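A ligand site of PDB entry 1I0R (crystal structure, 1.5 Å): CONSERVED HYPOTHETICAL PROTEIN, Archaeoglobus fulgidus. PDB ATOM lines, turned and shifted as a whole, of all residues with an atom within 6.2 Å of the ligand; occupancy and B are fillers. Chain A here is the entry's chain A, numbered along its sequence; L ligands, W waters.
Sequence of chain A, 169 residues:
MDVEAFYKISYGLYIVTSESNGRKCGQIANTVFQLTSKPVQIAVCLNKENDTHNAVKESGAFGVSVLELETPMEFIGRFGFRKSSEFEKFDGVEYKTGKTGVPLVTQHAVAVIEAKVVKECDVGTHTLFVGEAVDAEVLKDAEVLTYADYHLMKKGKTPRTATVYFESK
An oxygen (O9) of the ligand lies within hydrogen-bond range of the backbone NH (N) of Ser 84. An oxygen (O9) of the ligand is in hydrogen-bond range of the side-chain hydroxyl (OG) of Ser 84, at 2.6 Å. The backbone NH of Ile 28 is in hydrogen-bond range of an oxygen (O3) of the ligand (3.1 Å). The backbone carbonyl oxygen of Ile 28 is in hydrogen-bond range of an oxygen (O3) of the ligand, 2.8 Å away. O8 of the ligand is in hydrogen-bond range of N of Thr 52 (2.8 Å). O8 of the ligand sits at hydrogen-bond distance from OG1 of Thr 52. The backbone NH (N) of Asn 47 lies within hydrogen-bond range of an oxygen (O1) of the ligand, 2.8 Å away. The backbone carbonyl oxygen (O) of Arg 82 lies within hydrogen-bond range of an oxygen (O5) of the ligand (2.8 Å). N of Asp 51 is in hydrogen-bond range of O7 of the ligand (2.8 Å). The backbone NH (N) of Thr 31 sits at hydrogen-bond distance from an oxygen (O2) of the ligand (3.1 Å). The side-chain hydroxyl of Thr 31 sits at hydrogen-bond distance from an oxygen (O2) of the ligand (2.9 Å). NZ of Lys 89 is in salt-bridge range of O9 of the ligand (2.9 Å). O2 of the ligand sits at hydrogen-bond distance from N of Asn 30. N3 of the ligand lies close to OD1 of Asn 30 (3.0 Å). The backbone carbonyl oxygen (O) of Cys 45 is in hydrogen-bond range of a nitrogen (N2) of the ligand. A nitrogen (N1) of the ligand sits close to the side-chain amide oxygen (OE1) of Gln 27. OD1 of Asn 50 lies close to O1 of the ligand, 3.2 Å away.
N of Ser 84 sits at hydrogen-bond distance from OD1 of Asp 51, 3.4 Å away. The backbone NH (N) of Ile 28 is in hydrogen-bond range of the backbone carbonyl oxygen (O) of Phe 79 (3.4 Å). The side-chain amide oxygen (OD1) of Asn 47 is in hydrogen-bond range of the backbone NH (N) of Glu 49 (2.8 Å). The backbone carbonyl oxygen (O) of Arg 82 lies within hydrogen-bond range of the side-chain amino group (NZ) of Lys 89 (2.9 Å). OD1 of Asn 30 is in hydrogen-bond range of OG1 of Thr 31 (3.4 Å). The backbone NH of Cys 45 is in hydrogen-bond range of the backbone carbonyl oxygen of Thr 31. The side-chain amino group of Lys 89 lies within hydrogen-bond range of the backbone carbonyl oxygen of Phe 79, at 3.0 Å. A ring nitrogen (ND1) of His 53 sits at hydrogen-bond distance from the backbone carbonyl oxygen of Leu 46, at 3.4 Å.
Leu 13 touches the ligand (CD1 to C7, 3.7 Å). Gly 26 touches the ligand. Ala 29 touches the ligand (CA to N3, 3.4 Å). Leu 46 touches the ligand (CA to O1, 3.3 Å). Phe 79 touches the ligand. Gly 80 touches the ligand (O to C15, 3.4 Å). Phe 81 touches the ligand (CZ to C9, 3.6 Å). Lys 83 touches the ligand (C to O9, 3.6 Å). Tyr 147 touches the ligand (CE1 to C7, 3.9 Å). Tyr 150 touches the ligand (CE2 to C7, 3.4 Å). Hydrophobic or aromatic side chains that line the ligand: Leu 13, Ile 28, Ala 29, Phe 81, Tyr 147 and Tyr 150. Within 4 Å of the ligand: Leu 13, Gly 26, Gln 27, Ile 28, Ala 29, Asn 30, Thr 31, Cys 45, Leu 46, Asn 47, Asn 50, Asp 51, Thr 52, Phe 79, Gly 80, Phe 81, Arg 82, Lys 83, Ser 84, Lys 89, Tyr 147 and Tyr 150.
Water W2 lies within hydrogen-bond range of O7 of the ligand (2.5 Å), NZ of Lys 83 (2.8 Å) and ND2 of Asn 50 (3.3 Å). Water W1 lies within hydrogen-bond range of OD1 of Asn 30 (2.8 Å), O2 of the ligand (3.3 Å) and OG1 of Thr 31 (3.4 Å). Water W3 bridges a ring nitrogen (NE2) of His 126 (3.0 Å) and a nitrogen (N2) of the ligand (3.3 Å).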
ATOM      1  N   LEU A  13      11.560  -5.128  28.752  1.00  0.00           N
ATOM      2  CA  LEU A  13      11.481  -6.599  28.735  1.00  0.00           C
ATOM      3  C   LEU A  13      10.607  -6.956  29.939  1.00  0.00           C
ATOM      4  O   LEU A  13      10.816  -6.455  31.053  1.00  0.00           O
ATOM      5  CB  LEU A  13      12.855  -7.280  28.787  1.00  0.00           C
ATOM      6  CG  LEU A  13      12.751  -8.721  28.255  1.00  0.00           C
ATOM      7  CD1 LEU A  13      12.422  -8.699  26.776  1.00  0.00           C
ATOM      8  CD2 LEU A  13      14.090  -9.449  28.489  1.00  0.00           C
ATOM      9  N   CYS A  25       0.106 -19.589  33.167  1.00  0.00           N
ATOM     10  CA  CYS A  25       0.919 -19.391  31.975  1.00  0.00           C
ATOM     11  C   CYS A  25       1.686 -18.090  32.086  1.00  0.00           C
ATOM     12  O   CYS A  25       1.227 -17.094  32.652  1.00  0.00           O
ATOM     13  CB  CYS A  25       0.025 -19.280  30.727  1.00  0.00           C
ATOM     14  SG  CYS A  25      -0.883 -20.754  30.307  1.00  0.00           S
ATOM     15  N   GLY A  26       2.907 -18.107  31.542  1.00  0.00           N
ATOM     16  CA  GLY A  26       3.683 -16.882  31.535  1.00  0.00           C
ATOM     17  C   GLY A  26       4.656 -16.947  30.372  1.00  0.00           C
ATOM     18  O   GLY A  26       5.101 -18.018  29.950  1.00  0.00           O
ATOM     19  N   GLN A  27       5.019 -15.783  29.862  1.00  0.00           N
ATOM     20  CA  GLN A  27       5.959 -15.731  28.745  1.00  0.00           C
ATOM     21  C   GLN A  27       6.731 -14.432  28.792  1.00  0.00           C
ATOM     22  O   GLN A  27       6.309 -13.455  29.374  1.00  0.00           O
ATOM     23  CB  GLN A  27       5.218 -15.777  27.410  1.00  0.00           C
ATOM     24  CG  GLN A  27       4.273 -14.579  27.175  1.00  0.00           C
ATOM     25  CD  GLN A  27       3.939 -14.388  25.727  1.00  0.00           C
ATOM     26  OE1 GLN A  27       4.717 -13.740  24.966  1.00  0.00           O
ATOM     27  NE2 GLN A  27       2.831 -14.944  25.281  1.00  0.00           N
ATOM     28  N   ILE A  28       7.912 -14.426  28.180  1.00  0.00           N
ATOM     29  CA  ILE A  28       8.632 -13.159  28.070  1.00  0.00           C
ATOM     30  C   ILE A  28       7.971 -12.379  26.898  1.00  0.00           C
ATOM     31  O   ILE A  28       7.473 -12.955  25.920  1.00  0.00           O
ATOM     32  CB  ILE A  28      10.116 -13.406  27.682  1.00  0.00           C
ATOM     33  CG1 ILE A  28      10.825 -14.105  28.859  1.00  0.00           C
ATOM     34  CG2 ILE A  28      10.805 -12.044  27.307  1.00  0.00           C
ATOM     35  CD1 ILE A  28      11.056 -13.224  30.039  1.00  0.00           C
ATOM     36  N   ALA A  29       7.902 -11.063  27.040  1.00  0.00           N
ATOM     37  CA  ALA A  29       7.422 -10.193  25.944  1.00  0.00           C
ATOM     38  C   ALA A  29       8.169  -8.876  25.996  1.00  0.00           C
ATOM     39  O   ALA A  29       8.512  -8.380  27.081  1.00  0.00           O
ATOM     40  CB  ALA A  29       5.867  -9.889  26.095  1.00  0.00           C
ATOM     41  N   ASN A  30       8.472  -8.338  24.810  1.00  0.00           N
ATOM     42  CA  ASN A  30       9.016  -6.981  24.784  1.00  0.00           C
ATOM     43  C   ASN A  30       7.925  -6.019  24.305  1.00  0.00           C
ATOM     44  O   ASN A  30       8.011  -4.824  24.520  1.00  0.00           O
ATOM     45  CB  ASN A  30      10.300  -6.860  23.908  1.00  0.00           C
ATOM     46  CG  ASN A  30      10.096  -7.206  22.444  1.00  0.00           C
ATOM     47  OD1 ASN A  30       9.347  -8.106  22.092  1.00  0.00           O
ATOM     48  ND2 ASN A  30      10.811  -6.499  21.564  1.00  0.00           N
ATOM     49  N   THR A  31       6.866  -6.553  23.700  1.00  0.00           N
ATOM     50  CA  THR A  31       5.821  -5.688  23.129  1.00  0.00           C
ATOM     51  C   THR A  31       4.713  -5.388  24.121  1.00  0.00           C
ATOM     52  O   THR A  31       3.654  -6.012  24.074  1.00  0.00           O
ATOM     53  CB  THR A  31       5.239  -6.368  21.876  1.00  0.00           C
ATOM     54  OG1 THR A  31       6.318  -6.896  21.075  1.00  0.00           O
ATOM     55  CG2 THR A  31       4.477  -5.392  21.065  1.00  0.00           C
ATOM     56  N   VAL A  32       4.999  -4.479  25.048  1.00  0.00           N
ATOM     57  CA  VAL A  32       4.089  -4.077  26.129  1.00  0.00           C
ATOM     58  C   VAL A  32       4.168  -2.551  26.215  1.00  0.00           C
ATOM     59  O   VAL A  32       5.259  -2.008  26.342  1.00  0.00           O
ATOM     60  CB  VAL A  32       4.546  -4.655  27.514  1.00  0.00           C
ATOM     61  CG1 VAL A  32       3.682  -4.150  28.638  1.00  0.00           C
ATOM     62  CG2 VAL A  32       4.529  -6.184  27.439  1.00  0.00           C
ATOM     63  N   CYS A  45       1.168  -7.604  23.036  1.00  0.00           N
ATOM     64  CA  CYS A  45       0.960  -8.257  21.740  1.00  0.00           C
ATOM     65  C   CYS A  45       1.541  -9.665  21.815  1.00  0.00           C
ATOM     66  O   CYS A  45       2.766  -9.829  21.864  1.00  0.00           O
ATOM     67  CB  CYS A  45       1.639  -7.422  20.636  1.00  0.00           C
ATOM     68  SG  CYS A  45       1.065  -7.930  19.007  1.00  0.00           S
ATOM     69  N   LEU A  46       0.649 -10.664  21.825  1.00  0.00           N
ATOM     70  CA  LEU A  46       1.043 -12.055  22.015  1.00  0.00           C
ATOM     71  C   LEU A  46       0.781 -12.927  20.806  1.00  0.00           C
ATOM     72  O   LEU A  46      -0.277 -12.840  20.194  1.00  0.00           O
ATOM     73  CB  LEU A  46       0.262 -12.642  23.213  1.00  0.00           C
ATOM     74  CG  LEU A  46       0.272 -11.816  24.494  1.00  0.00           C
ATOM     75  CD1 LEU A  46      -0.431 -12.630  25.593  1.00  0.00           C
ATOM     76  CD2 LEU A  46       1.746 -11.491  24.922  1.00  0.00           C
ATOM     77  N   ASN A  47       1.743 -13.788  20.485  1.00  0.00           N
ATOM     78  CA  ASN A  47       1.628 -14.676  19.339  1.00  0.00           C
ATOM     79  C   ASN A  47       0.507 -15.717  19.591  1.00  0.00           C
ATOM     80  O   ASN A  47       0.431 -16.284  20.691  1.00  0.00           O
ATOM     81  CB  ASN A  47       2.994 -15.383  19.099  1.00  0.00           C
ATOM     82  CG  ASN A  47       3.016 -16.170  17.799  1.00  0.00           C
ATOM     83  OD1 ASN A  47       2.222 -17.083  17.609  1.00  0.00           O
ATOM     84  ND2 ASN A  47       3.933 -15.808  16.881  1.00  0.00           N
ATOM     85  N   LYS A  48      -0.365 -15.917  18.603  1.00  0.00           N
ATOM     86  CA  LYS A  48      -1.478 -16.877  18.734  1.00  0.00           C
ATOM     87  C   LYS A  48      -1.048 -18.318  19.076  1.00  0.00           C
ATOM     88  O   LYS A  48      -1.855 -19.097  19.586  1.00  0.00           O
ATOM     89  CB  LYS A  48      -2.312 -16.865  17.456  1.00  0.00           C
ATOM     90  CG  LYS A  48      -3.064 -15.562  17.238  1.00  0.00           C
ATOM     91  CD  LYS A  48      -3.840 -15.591  15.918  1.00  0.00           C
ATOM     92  CE  LYS A  48      -4.611 -14.290  15.731  1.00  0.00           C
ATOM     93  NZ  LYS A  48      -5.324 -14.322  14.422  1.00  0.00           N
ATOM     94  N   GLU A  49       0.201 -18.663  18.798  1.00  0.00           N
ATOM     95  CA  GLU A  49       0.690 -20.018  19.117  1.00  0.00           C
ATOM     96  C   GLU A  49       1.030 -20.200  20.600  1.00  0.00           C
ATOM     97  O   GLU A  49       1.196 -21.349  21.077  1.00  0.00           O
ATOM     98  CB  GLU A  49       1.946 -20.318  18.277  1.00  0.00           C
ATOM     99  CG  GLU A  49       1.661 -20.522  16.803  1.00  0.00           C
ATOM    100  CD  GLU A  49       2.924 -20.599  15.948  1.00  0.00           C
ATOM    101  OE1 GLU A  49       4.044 -20.681  16.511  1.00  0.00           O
ATOM    102  OE2 GLU A  49       2.801 -20.580  14.704  1.00  0.00           O
ATOM    103  N   ASN A  50       1.123 -19.101  21.350  1.00  0.00           N
ATOM    104  CA  ASN A  50       1.545 -19.169  22.734  1.00  0.00           C
ATOM    105  C   ASN A  50       0.506 -19.629  23.713  1.00  0.00           C
ATOM    106  O   ASN A  50      -0.663 -19.218  23.626  1.00  0.00           O
ATOM    107  CB  ASN A  50       2.018 -17.788  23.227  1.00  0.00           C
ATOM    108  CG  ASN A  50       3.244 -17.258  22.486  1.00  0.00           C
ATOM    109  OD1 ASN A  50       3.671 -16.128  22.742  1.00  0.00           O
ATOM    110  ND2 ASN A  50       3.808 -18.054  21.597  1.00  0.00           N
ATOM    111  N   ASP A  51       0.920 -20.445  24.677  1.00  0.00           N
ATOM    112  CA  ASP A  51      -0.014 -20.854  25.727  1.00  0.00           C
ATOM    113  C   ASP A  51      -0.540 -19.619  26.480  1.00  0.00           C
ATOM    114  O   ASP A  51      -1.721 -19.573  26.856  1.00  0.00           O
ATOM    115  CB  ASP A  51       0.654 -21.835  26.722  1.00  0.00           C
ATOM    116  CG  ASP A  51       0.805 -23.224  26.130  1.00  0.00           C
ATOM    117  OD1 ASP A  51       1.717 -23.959  26.611  1.00  0.00           O
ATOM    118  OD2 ASP A  51       0.054 -23.612  25.182  1.00  0.00           O
ATOM    119  N   THR A  52       0.291 -18.600  26.715  1.00  0.00           N
ATOM    120  CA  THR A  52      -0.137 -17.420  27.464  1.00  0.00           C
ATOM    121  C   THR A  52      -1.198 -16.649  26.654  1.00  0.00           C
ATOM    122  O   THR A  52      -2.164 -16.121  27.259  1.00  0.00           O
ATOM    123  CB  THR A  52       1.044 -16.490  27.839  1.00  0.00           C
ATOM    124  OG1 THR A  52       2.035 -17.260  28.552  1.00  0.00           O
ATOM    125  CG2 THR A  52       0.554 -15.341  28.755  1.00  0.00           C
ATOM    126  N   HIS A  53      -1.046 -16.611  25.330  1.00  0.00           N
ATOM    127  CA  HIS A  53      -2.068 -15.971  24.471  1.00  0.00           C
ATOM    128  C   HIS A  53      -3.436 -16.600  24.707  1.00  0.00           C
ATOM    129  O   HIS A  53      -4.440 -15.902  24.892  1.00  0.00           O
ATOM    130  CB  HIS A  53      -1.673 -16.123  22.991  1.00  0.00           C
ATOM    131  CG  HIS A  53      -2.793 -15.860  22.034  1.00  0.00           C
ATOM    132  ND1 HIS A  53      -2.950 -14.670  21.349  1.00  0.00           N
ATOM    133  CD2 HIS A  53      -3.831 -16.643  21.666  1.00  0.00           C
ATOM    134  CE1 HIS A  53      -4.036 -14.737  20.594  1.00  0.00           C
ATOM    135  NE2 HIS A  53      -4.589 -15.927  20.765  1.00  0.00           N
ATOM    136  N   ILE A  76      15.137 -15.535  32.223  1.00  0.00           N
ATOM    137  CA  ILE A  76      14.485 -15.100  30.976  1.00  0.00           C
ATOM    138  C   ILE A  76      14.201 -16.343  30.123  1.00  0.00           C
ATOM    139  O   ILE A  76      13.127 -16.470  29.507  1.00  0.00           O
ATOM    140  CB  ILE A  76      15.402 -14.092  30.216  1.00  0.00           C
ATOM    141  CG1 ILE A  76      15.466 -12.802  31.024  1.00  0.00           C
ATOM    142  CG2 ILE A  76      14.919 -13.845  28.791  1.00  0.00           C
ATOM    143  CD1 ILE A  76      16.596 -11.847  30.547  1.00  0.00           C
ATOM    144  N   PHE A  79      11.109 -18.473  31.048  1.00  0.00           N
ATOM    145  CA  PHE A  79       9.830 -17.983  30.522  1.00  0.00           C
ATOM    146  C   PHE A  79       9.734 -17.764  29.037  1.00  0.00           C
ATOM    147  O   PHE A  79       8.637 -17.776  28.467  1.00  0.00           O
ATOM    148  CB  PHE A  79       9.423 -16.658  31.212  1.00  0.00           C
ATOM    149  CG  PHE A  79       8.939 -16.832  32.630  1.00  0.00           C
ATOM    150  CD1 PHE A  79       9.799 -16.686  33.696  1.00  0.00           C
ATOM    151  CD2 PHE A  79       7.607 -17.196  32.897  1.00  0.00           C
ATOM    152  CE1 PHE A  79       9.390 -16.897  35.011  1.00  0.00           C
ATOM    153  CE2 PHE A  79       7.163 -17.422  34.227  1.00  0.00           C
ATOM    154  CZ  PHE A  79       8.065 -17.273  35.274  1.00  0.00           C
ATOM    155  N   GLY A  80      10.874 -17.585  28.383  1.00  0.00           N
ATOM    156  CA  GLY A  80      10.862 -17.254  26.978  1.00  0.00           C
ATOM    157  C   GLY A  80      11.259 -18.268  25.912  1.00  0.00           C
ATOM    158  O   GLY A  80      11.171 -17.986  24.709  1.00  0.00           O
ATOM    159  N   PHE A  81      11.663 -19.455  26.354  1.00  0.00           N
ATOM    160  CA  PHE A  81      12.098 -20.478  25.413  1.00  0.00           C
ATOM    161  C   PHE A  81      11.477 -21.847  25.599  1.00  0.00           C
ATOM    162  O   PHE A  81      12.067 -22.870  25.218  1.00  0.00           O
ATOM    163  CB  PHE A  81      13.647 -20.581  25.438  1.00  0.00           C
ATOM    164  CG  PHE A  81      14.344 -19.377  24.857  1.00  0.00           C
ATOM    165  CD1 PHE A  81      14.972 -18.468  25.690  1.00  0.00           C
ATOM    166  CD2 PHE A  81      14.283 -19.112  23.502  1.00  0.00           C
ATOM    167  CE1 PHE A  81      15.522 -17.281  25.183  1.00  0.00           C
ATOM    168  CE2 PHE A  81      14.833 -17.922  22.986  1.00  0.00           C
ATOM    169  CZ  PHE A  81      15.450 -17.015  23.839  1.00  0.00           C
ATOM    170  N   ARG A  82      10.268 -21.863  26.165  1.00  0.00           N
ATOM    171  CA  ARG A  82       9.553 -23.130  26.339  1.00  0.00           C
ATOM    172  C   ARG A  82       8.072 -22.805  26.551  1.00  0.00           C
ATOM    173  O   ARG A  82       7.718 -21.638  26.776  1.00  0.00           O
ATOM    174  CB  ARG A  82      10.106 -23.924  27.534  1.00  0.00           C
ATOM    175  CG  ARG A  82       9.917 -23.238  28.882  1.00  0.00           C
ATOM    176  CD  ARG A  82      10.993 -23.645  29.888  1.00  0.00           C
ATOM    177  NE  ARG A  82      12.269 -23.017  29.544  1.00  0.00           N
ATOM    178  CZ  ARG A  82      13.470 -23.532  29.819  1.00  0.00           C
ATOM    179  NH1 ARG A  82      13.562 -24.713  30.442  1.00  0.00           N
ATOM    180  NH2 ARG A  82      14.582 -22.881  29.447  1.00  0.00           N
ATOM    181  N   LYS A  83       7.210 -23.820  26.474  1.00  0.00           N
ATOM    182  CA  LYS A  83       5.752 -23.574  26.632  1.00  0.00           C
ATOM    183  C   LYS A  83       5.264 -23.857  28.048  1.00  0.00           C
ATOM    184  O   LYS A  83       5.680 -24.856  28.684  1.00  0.00           O
ATOM    185  CB  LYS A  83       4.958 -24.450  25.667  1.00  0.00           C
ATOM    186  CG  LYS A  83       5.238 -24.185  24.219  1.00  0.00           C
ATOM    187  CD  LYS A  83       4.365 -25.060  23.336  1.00  0.00           C
ATOM    188  CE  LYS A  83       4.494 -24.636  21.869  1.00  0.00           C
ATOM    189  NZ  LYS A  83       3.659 -23.418  21.591  1.00  0.00           N
ATOM    190  N   SER A  84       4.376 -22.995  28.528  1.00  0.00           N
ATOM    191  CA  SER A  84       3.806 -23.097  29.882  1.00  0.00           C
ATOM    192  C   SER A  84       3.097 -24.429  30.151  1.00  0.00           C
ATOM    193  O   SER A  84       3.123 -24.919  31.278  1.00  0.00           O
ATOM    194  CB  SER A  84       2.784 -21.982  30.133  1.00  0.00           C
ATOM    195  OG  SER A  84       3.377 -20.704  30.126  1.00  0.00           O
ATOM    196  N   SER A  85       2.503 -24.996  29.110  1.00  0.00           N
ATOM    197  CA  SER A  85       1.777 -26.257  29.243  1.00  0.00           C
ATOM    198  C   SER A  85       2.705 -27.463  29.276  1.00  0.00           C
ATOM    199  O   SER A  85       2.268 -28.561  29.625  1.00  0.00           O
ATOM    200  CB  SER A  85       0.783 -26.443  28.099  1.00  0.00           C
ATOM    201  OG  SER A  85       1.434 -26.570  26.854  1.00  0.00           O
ATOM    202  N   LYS A  89       6.764 -23.538  34.599  1.00  0.00           N
ATOM    203  CA  LYS A  89       7.506 -22.282  34.706  1.00  0.00           C
ATOM    204  C   LYS A  89       7.466 -21.591  36.048  1.00  0.00           C
ATOM    205  O   LYS A  89       8.424 -20.895  36.428  1.00  0.00           O
ATOM    206  CB  LYS A  89       6.995 -21.288  33.636  1.00  0.00           C
ATOM    207  CG  LYS A  89       7.289 -21.695  32.200  1.00  0.00           C
ATOM    208  CD  LYS A  89       6.757 -20.658  31.227  1.00  0.00           C
ATOM    209  CE  LYS A  89       7.209 -20.977  29.833  1.00  0.00           C
ATOM    210  NZ  LYS A  89       6.626 -19.995  28.841  1.00  0.00           N
ATOM    211  N   HIS A 126      -0.633 -12.586  15.592  1.00  0.00           N
ATOM    212  CA  HIS A 126      -0.702 -12.196  17.008  1.00  0.00           C
ATOM    213  C   HIS A 126      -2.034 -11.525  17.290  1.00  0.00           C
ATOM    214  O   HIS A 126      -2.714 -11.051  16.369  1.00  0.00           O
ATOM    215  CB  HIS A 126       0.346 -11.112  17.322  1.00  0.00           C
ATOM    216  CG  HIS A 126       1.781 -11.582  17.273  1.00  0.00           C
ATOM    217  ND1 HIS A 126       2.363 -12.109  16.143  1.00  0.00           N
ATOM    218  CD2 HIS A 126       2.754 -11.549  18.223  1.00  0.00           C
ATOM    219  CE1 HIS A 126       3.633 -12.375  16.393  1.00  0.00           C
ATOM    220  NE2 HIS A 126       3.890 -12.045  17.643  1.00  0.00           N
ATOM    221  N   TYR A 147      15.136  -3.968  26.150  1.00  0.00           N
ATOM    222  CA  TYR A 147      15.342  -4.999  25.137  1.00  0.00           C
ATOM    223  C   TYR A 147      16.748  -4.822  24.543  1.00  0.00           C
ATOM    224  O   TYR A 147      17.443  -5.802  24.261  1.00  0.00           O
ATOM    225  CB  TYR A 147      14.230  -4.881  24.072  1.00  0.00           C
ATOM    226  CG  TYR A 147      14.286  -5.941  23.003  1.00  0.00           C
ATOM    227  CD1 TYR A 147      14.155  -7.292  23.325  1.00  0.00           C
ATOM    228  CD2 TYR A 147      14.433  -5.587  21.661  1.00  0.00           C
ATOM    229  CE1 TYR A 147      14.180  -8.261  22.315  1.00  0.00           C
ATOM    230  CE2 TYR A 147      14.459  -6.556  20.651  1.00  0.00           C
ATOM    231  CZ  TYR A 147      14.337  -7.882  20.992  1.00  0.00           C
ATOM    232  OH  TYR A 147      14.413  -8.833  20.010  1.00  0.00           O
ATOM    233  N   TYR A 150      19.196  -6.405  26.808  1.00  0.00           N
ATOM    234  CA  TYR A 150      19.170  -7.847  26.645  1.00  0.00           C
ATOM    235  C   TYR A 150      20.002  -8.267  25.431  1.00  0.00           C
ATOM    236  O   TYR A 150      20.681  -9.300  25.467  1.00  0.00           O
ATOM    237  CB  TYR A 150      17.711  -8.324  26.538  1.00  0.00           C
ATOM    238  CG  TYR A 150      17.544  -9.695  25.994  1.00  0.00           C
ATOM    239  CD1 TYR A 150      17.755 -10.810  26.798  1.00  0.00           C
ATOM    240  CD2 TYR A 150      17.179  -9.886  24.668  1.00  0.00           C
ATOM    241  CE1 TYR A 150      17.585 -12.100  26.279  1.00  0.00           C
ATOM    242  CE2 TYR A 150      17.016 -11.149  24.127  1.00  0.00           C
ATOM    243  CZ  TYR A 150      17.220 -12.257  24.953  1.00  0.00           C
ATOM    244  OH  TYR A 150      17.069 -13.515  24.414  1.00  0.00           O
HETATM  245  N1  LIG L   1       6.323 -13.473  22.281  1.00  0.00           N
HETATM  246  C1  LIG L   1       5.249 -12.699  22.027  1.00  0.00           C
HETATM  247  O1  LIG L   1       4.144 -13.156  21.748  1.00  0.00           O
HETATM  248  N2  LIG L   1       5.407 -11.295  22.130  1.00  0.00           N
HETATM  249  C2  LIG L   1       6.589 -10.637  22.421  1.00  0.00           C
HETATM  250  O2  LIG L   1       6.617  -9.400  22.500  1.00  0.00           O
HETATM  251  C3  LIG L   1       7.726 -11.472  22.658  1.00  0.00           C
HETATM  252  N3  LIG L   1       8.919 -10.943  22.962  1.00  0.00           N
HETATM  253  C4  LIG L   1       9.939 -11.807  23.312  1.00  0.00           C
HETATM  254  C5  LIG L   1      11.222 -11.281  23.702  1.00  0.00           C
HETATM  255  C6  LIG L   1      12.265 -12.051  24.113  1.00  0.00           C
HETATM  256  C7  LIG L   1      13.608 -11.445  24.529  1.00  0.00           C
HETATM  257  C8  LIG L   1      12.086 -13.503  24.215  1.00  0.00           C
HETATM  258  C9  LIG L   1      13.180 -14.396  24.715  1.00  0.00           C
HETATM  259  C10 LIG L   1      10.861 -14.037  23.793  1.00  0.00           C
HETATM  260  C11 LIG L   1       9.790 -13.244  23.335  1.00  0.00           C
HETATM  261  N4  LIG L   1       8.546 -13.736  22.905  1.00  0.00           N
HETATM  262  C12 LIG L   1       7.494 -12.921  22.602  1.00  0.00           C
HETATM  263  C13 LIG L   1       8.328 -15.207  22.832  1.00  0.00           C
HETATM  264  C14 LIG L   1       7.682 -15.897  24.034  1.00  0.00           C
HETATM  265  O3  LIG L   1       8.286 -15.504  25.262  1.00  0.00           O
HETATM  266  C15 LIG L   1       7.906 -17.408  23.847  1.00  0.00           C
HETATM  267  O4  LIG L   1       7.376 -17.856  22.572  1.00  0.00           O
HETATM  268  C16 LIG L   1       7.369 -18.238  24.988  1.00  0.00           C
HETATM  269  O5  LIG L   1       7.940 -19.569  24.866  1.00  0.00           O
HETATM  270  C17 LIG L   1       5.881 -18.370  24.975  1.00  0.00           C
HETATM  271  O6  LIG L   1       5.503 -19.159  26.092  1.00  0.00           O
HETATM  272  P1  LIG L   1       3.995 -19.718  26.261  1.00  0.00           P
HETATM  273  O7  LIG L   1       3.713 -20.596  25.092  1.00  0.00           O
HETATM  274  O8  LIG L   1       3.062 -18.515  26.311  1.00  0.00           O
HETATM  275  O9  LIG L   1       4.058 -20.494  27.584  1.00  0.00           O
HETATM  276  O   HOH W   1       8.400  -9.288  19.761  1.00  0.00           O
HETATM  277  O   HOH W   2       4.652 -21.031  22.766  1.00  0.00           O
HETATM  278  O   HOH W   3       6.491 -11.498  18.990  1.00  0.00           O
HETATM  279  O   HOH W   4       9.406 -18.484  20.775  1.00  0.00           O
